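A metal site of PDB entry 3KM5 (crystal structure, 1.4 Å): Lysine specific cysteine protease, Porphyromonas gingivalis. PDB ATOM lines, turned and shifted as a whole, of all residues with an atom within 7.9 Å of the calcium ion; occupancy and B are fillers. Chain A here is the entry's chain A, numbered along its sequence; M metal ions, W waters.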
ATOM      1  N   GLU A   7     -23.135  11.553 -31.583  1.00  0.00           N
ATOM      2  CA  GLU A   7     -22.932  10.998 -30.255  1.00  0.00           C
ATOM      3  C   GLU A   7     -23.911   9.870 -30.002  1.00  0.00           C
ATOM      4  O   GLU A   7     -25.124  10.089 -30.040  1.00  0.00           O
ATOM      5  CB  GLU A   7     -23.079  12.073 -29.168  1.00  0.00           C
ATOM      6  CG  GLU A   7     -23.005  11.529 -27.754  1.00  0.00           C
ATOM      7  CD  GLU A   7     -21.668  10.861 -27.476  1.00  0.00           C
ATOM      8  OE1 GLU A   7     -20.659  11.605 -27.372  1.00  0.00           O
ATOM      9  OE2 GLU A   7     -21.628   9.622 -27.380  1.00  0.00           O
ATOM     10  N   THR A   8     -23.386   8.657 -29.842  1.00  0.00           N
ATOM     11  CA  THR A   8     -24.220   7.468 -29.648  1.00  0.00           C
ATOM     12  C   THR A   8     -24.270   7.029 -28.206  1.00  0.00           C
ATOM     13  O   THR A   8     -25.048   6.147 -27.882  1.00  0.00           O
ATOM     14  CB  THR A   8     -23.701   6.290 -30.467  1.00  0.00           C
ATOM     15  OG1 THR A   8     -22.421   5.888 -29.968  1.00  0.00           O
ATOM     16  CG2 THR A   8     -23.658   6.652 -31.956  1.00  0.00           C
ATOM     17  N   PHE A   9     -23.364   7.564 -27.392  1.00  0.00           N
ATOM     18  CA  PHE A   9     -23.168   7.126 -26.003  1.00  0.00           C
ATOM     19  C   PHE A   9     -22.638   5.713 -25.855  1.00  0.00           C
ATOM     20  O   PHE A   9     -22.468   5.251 -24.747  1.00  0.00           O
ATOM     21  CB  PHE A   9     -24.410   7.357 -25.138  1.00  0.00           C
ATOM     22  CG  PHE A   9     -24.827   8.800 -25.116  1.00  0.00           C
ATOM     23  CD1 PHE A   9     -24.015   9.738 -24.498  1.00  0.00           C
ATOM     24  CD2 PHE A   9     -25.930   9.226 -25.847  1.00  0.00           C
ATOM     25  CE1 PHE A   9     -24.320  11.095 -24.551  1.00  0.00           C
ATOM     26  CE2 PHE A   9     -26.233  10.594 -25.887  1.00  0.00           C
ATOM     27  CZ  PHE A   9     -25.442  11.513 -25.253  1.00  0.00           C
ATOM     28  N   GLU A  10     -22.284   5.064 -26.957  1.00  0.00           N
ATOM     29  CA  GLU A  10     -21.827   3.689 -26.893  1.00  0.00           C
ATOM     30  C   GLU A  10     -20.441   3.593 -26.250  1.00  0.00           C
ATOM     31  O   GLU A  10     -20.160   2.572 -25.601  1.00  0.00           O
ATOM     32  CB  GLU A  10     -21.864   3.028 -28.269  1.00  0.00           C
ATOM     33  CG  GLU A  10     -23.261   3.035 -28.871  1.00  0.00           C
ATOM     34  CD  GLU A  10     -24.297   2.401 -27.996  1.00  0.00           C
ATOM     35  OE1 GLU A  10     -24.121   1.234 -27.555  1.00  0.00           O
ATOM     36  OE2 GLU A  10     -25.360   3.049 -27.751  1.00  0.00           O
ATOM     37  N   SER A  11     -19.634   4.654 -26.395  1.00  0.00           N
ATOM     38  CA  SER A  11     -18.318   4.722 -25.722  1.00  0.00           C
ATOM     39  C   SER A  11     -18.357   5.184 -24.248  1.00  0.00           C
ATOM     40  O   SER A  11     -17.310   5.261 -23.598  1.00  0.00           O
ATOM     41  CB  SER A  11     -17.365   5.618 -26.487  1.00  0.00           C
ATOM     42  OG  SER A  11     -17.653   6.982 -26.248  1.00  0.00           O
ATOM     43  N   LEU A  36     -26.890   5.530 -19.346  1.00  0.00           N
ATOM     44  CA  LEU A  36     -27.525   4.267 -18.951  1.00  0.00           C
ATOM     45  C   LEU A  36     -27.337   3.235 -20.056  1.00  0.00           C
ATOM     46  O   LEU A  36     -27.387   3.590 -21.246  1.00  0.00           O
ATOM     47  CB  LEU A  36     -29.017   4.430 -18.757  1.00  0.00           C
ATOM     48  CG  LEU A  36     -29.471   5.509 -17.777  1.00  0.00           C
ATOM     49  CD1 LEU A  36     -31.012   5.563 -17.751  1.00  0.00           C
ATOM     50  CD2 LEU A  36     -28.864   5.346 -16.375  1.00  0.00           C
ATOM     51  N   ALA A  46     -32.328   1.351 -25.796  1.00  0.00           N
ATOM     52  CA  ALA A  46     -31.739   2.529 -26.465  1.00  0.00           C
ATOM     53  C   ALA A  46     -32.310   2.717 -27.843  1.00  0.00           C
ATOM     54  O   ALA A  46     -32.834   1.766 -28.448  1.00  0.00           O
ATOM     55  CB  ALA A  46     -30.225   2.359 -26.559  1.00  0.00           C
ATOM     56  N   HIS A  47     -32.143   3.932 -28.368  1.00  0.00           N
ATOM     57  CA  HIS A  47     -32.556   4.186 -29.751  1.00  0.00           C
ATOM     58  C   HIS A  47     -31.611   3.447 -30.704  1.00  0.00           C
ATOM     59  O   HIS A  47     -32.034   2.849 -31.692  1.00  0.00           O
ATOM     60  CB  HIS A  47     -32.488   5.671 -30.080  1.00  0.00           C
ATOM     61  CG  HIS A  47     -32.917   5.977 -31.469  1.00  0.00           C
ATOM     62  ND1 HIS A  47     -32.053   6.402 -32.450  1.00  0.00           N
ATOM     63  CD2 HIS A  47     -34.136   5.892 -32.052  1.00  0.00           C
ATOM     64  CE1 HIS A  47     -32.713   6.548 -33.593  1.00  0.00           C
ATOM     65  NE2 HIS A  47     -33.983   6.276 -33.361  1.00  0.00           N
ATOM     66  N   GLY A  48     -30.318   3.531 -30.392  1.00  0.00           N
ATOM     67  CA  GLY A  48     -29.309   2.769 -31.100  1.00  0.00           C
ATOM     68  C   GLY A  48     -28.323   2.115 -30.152  1.00  0.00           C
ATOM     69  O   GLY A  48     -28.002   2.647 -29.114  1.00  0.00           O
ATOM     70  N   GLY A  49     -27.825   0.919 -30.483  1.00  0.00           N
ATOM     71  CA  GLY A  49     -26.919   0.235 -29.574  1.00  0.00           C
ATOM     72  C   GLY A  49     -27.522  -0.062 -28.220  1.00  0.00           C
ATOM     73  O   GLY A  49     -28.732  -0.337 -28.155  1.00  0.00           O
ATOM     74  N   SER A  50     -26.700  -0.013 -27.167  1.00  0.00           N
ATOM     75  CA  SER A  50     -27.193  -0.324 -25.827  1.00  0.00           C
ATOM     76  C   SER A  50     -27.322   0.895 -24.926  1.00  0.00           C
ATOM     77  O   SER A  50     -28.018   0.844 -23.900  1.00  0.00           O
ATOM     78  CB  SER A  50     -26.319  -1.369 -25.125  1.00  0.00           C
ATOM     79  OG  SER A  50     -25.040  -0.859 -24.806  1.00  0.00           O
ATOM     80  N   ASN A  51     -26.686   2.003 -25.310  1.00  0.00           N
ATOM     81  CA  ASN A  51     -26.546   3.150 -24.388  1.00  0.00           C
ATOM     82  C   ASN A  51     -27.346   4.405 -24.758  1.00  0.00           C
ATOM     83  O   ASN A  51     -27.492   4.765 -25.919  1.00  0.00           O
ATOM     84  CB  ASN A  51     -25.076   3.532 -24.272  1.00  0.00           C
ATOM     85  CG  ASN A  51     -24.233   2.480 -23.514  1.00  0.00           C
ATOM     86  OD1 ASN A  51     -24.740   1.446 -23.145  1.00  0.00           O
ATOM     87  ND2 ASN A  51     -22.990   2.776 -23.281  1.00  0.00           N
ATOM     88  N   VAL A  52     -27.806   5.081 -23.728  1.00  0.00           N
ATOM     89  CA  VAL A  52     -28.417   6.430 -23.868  1.00  0.00           C
ATOM     90  C   VAL A  52     -27.804   7.359 -22.832  1.00  0.00           C
ATOM     91  O   VAL A  52     -27.029   6.927 -22.004  1.00  0.00           O
ATOM     92  CB  VAL A  52     -29.943   6.353 -23.646  1.00  0.00           C
ATOM     93  CG1 VAL A  52     -30.562   5.307 -24.617  1.00  0.00           C
ATOM     94  CG2 VAL A  52     -30.225   6.014 -22.177  1.00  0.00           C
ATOM     95  N   VAL A  53     -28.204   8.630 -22.842  1.00  0.00           N
ATOM     96  CA  VAL A  53     -27.987   9.507 -21.680  1.00  0.00           C
ATOM     97  C   VAL A  53     -29.376   9.855 -21.071  1.00  0.00           C
ATOM     98  O   VAL A  53     -30.378   9.900 -21.801  1.00  0.00           O
ATOM     99  CB  VAL A  53     -27.156  10.743 -22.049  1.00  0.00           C
ATOM    100  CG1 VAL A  53     -27.982  11.760 -22.875  1.00  0.00           C
ATOM    101  CG2 VAL A  53     -26.481  11.384 -20.823  1.00  0.00           C
ATOM    102  N   TRP A 142     -39.348   6.694 -29.253  1.00  0.00           N
ATOM    103  CA  TRP A 142     -38.261   7.657 -29.618  1.00  0.00           C
ATOM    104  C   TRP A 142     -38.744   8.656 -30.652  1.00  0.00           C
ATOM    105  O   TRP A 142     -39.297   8.287 -31.683  1.00  0.00           O
ATOM    106  CB  TRP A 142     -37.045   6.912 -30.175  1.00  0.00           C
ATOM    107  CG  TRP A 142     -36.376   6.181 -29.104  1.00  0.00           C
ATOM    108  CD1 TRP A 142     -36.612   4.878 -28.714  1.00  0.00           C
ATOM    109  CD2 TRP A 142     -35.403   6.698 -28.200  1.00  0.00           C
ATOM    110  NE1 TRP A 142     -35.803   4.562 -27.656  1.00  0.00           N
ATOM    111  CE2 TRP A 142     -35.099   5.675 -27.286  1.00  0.00           C
ATOM    112  CE3 TRP A 142     -34.804   7.936 -28.048  1.00  0.00           C
ATOM    113  CZ2 TRP A 142     -34.167   5.837 -26.265  1.00  0.00           C
ATOM    114  CZ3 TRP A 142     -33.871   8.098 -27.026  1.00  0.00           C
ATOM    115  CH2 TRP A 142     -33.560   7.052 -26.164  1.00  0.00           C
ATOM    116  N   LEU A 171     -31.845  10.758 -24.150  1.00  0.00           N
ATOM    117  CA  LEU A 171     -31.382  11.226 -25.455  1.00  0.00           C
ATOM    118  C   LEU A 171     -30.477  10.187 -26.049  1.00  0.00           C
ATOM    119  O   LEU A 171     -29.769   9.500 -25.325  1.00  0.00           O
ATOM    120  CB  LEU A 171     -30.616  12.564 -25.393  1.00  0.00           C
ATOM    121  CG  LEU A 171     -31.322  13.688 -24.686  1.00  0.00           C
ATOM    122  CD1 LEU A 171     -30.379  14.855 -24.412  1.00  0.00           C
ATOM    123  CD2 LEU A 171     -32.495  14.198 -25.513  1.00  0.00           C
ATOM    124  N   ASP A 172     -30.496  10.101 -27.366  1.00  0.00           N
ATOM    125  CA  ASP A 172     -29.543   9.218 -28.066  1.00  0.00           C
ATOM    126  C   ASP A 172     -29.353   9.739 -29.493  1.00  0.00           C
ATOM    127  O   ASP A 172     -30.136  10.498 -30.007  1.00  0.00           O
ATOM    128  CB  ASP A 172     -30.103   7.800 -28.030  1.00  0.00           C
ATOM    129  CG  ASP A 172     -29.053   6.709 -28.275  1.00  0.00           C
ATOM    130  OD1 ASP A 172     -27.855   7.034 -28.336  1.00  0.00           O
ATOM    131  OD2 ASP A 172     -29.462   5.524 -28.306  1.00  0.00           O
ATOM    132  N   ASP A 173     -28.256   9.306 -30.101  1.00  0.00           N
ATOM    133  CA  ASP A 173     -27.985   9.543 -31.510  1.00  0.00           C
ATOM    134  C   ASP A 173     -28.067  11.033 -31.855  1.00  0.00           C
ATOM    135  O   ASP A 173     -28.792  11.479 -32.765  1.00  0.00           O
ATOM    136  CB  ASP A 173     -28.883   8.642 -32.405  1.00  0.00           C
ATOM    137  CG  ASP A 173     -28.463   7.194 -32.341  1.00  0.00           C
ATOM    138  OD1 ASP A 173     -27.267   6.929 -32.141  1.00  0.00           O
ATOM    139  OD2 ASP A 173     -29.333   6.291 -32.390  1.00  0.00           O
ATOM    140  N   ILE A 174     -27.267  11.800 -31.125  1.00  0.00           N
ATOM    141  CA  ILE A 174     -27.216  13.241 -31.292  1.00  0.00           C
ATOM    142  C   ILE A 174     -26.203  13.622 -32.397  1.00  0.00           C
ATOM    143  O   ILE A 174     -24.977  13.502 -32.190  1.00  0.00           O
ATOM    144  CB  ILE A 174     -26.796  13.959 -29.969  1.00  0.00           C
ATOM    145  CG1 ILE A 174     -27.687  13.499 -28.809  1.00  0.00           C
ATOM    146  CG2 ILE A 174     -26.799  15.465 -30.178  1.00  0.00           C
ATOM    147  CD1 ILE A 174     -27.151  13.942 -27.470  1.00  0.00           C
HETATM  148 CA    CA M   1     -26.983   4.717 -28.231  1.00  0.00          CA
HETATM  149  O   HOH W   1     -26.713   4.925 -30.567  1.00  0.00           O
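The calcium ion is bound by water W1, 2.4 Å away.
The calcium ion is bound by the backbone carbonyl oxygen (O) of Asn 51.
The calcium ion is bound by OE2 of Glu 10.
O of Thr 8 is bound to the calcium ion (2.4 Å).
O of Gly 48 is bound to the calcium ion (2.5 Å).
The calcium ion is bound by the side-chain carboxylate (OD1) of Asp 172, 2.5 Å away.
OD2 of Asp 172 binds the calcium ion (2.6 Å).
The calcium ion has seven donor atoms within binding distance.
Along chain A the residues within 4 Å of the calcium ion span positions 8 to 172.
OG of Ser 50 is in hydrogen-bond range of OD1 of Asn 51.
O of Phe 9 lies within hydrogen-bond range of ND2 of Asn 51 (2.9 Å).
The backbone NH (N) of His 47 lies close to the side-chain carboxylate (OD2) of Asp 172 (3.1 Å).
OE1 of Glu 10 is in hydrogen-bond range of N of Ser 50 (2.9 Å).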
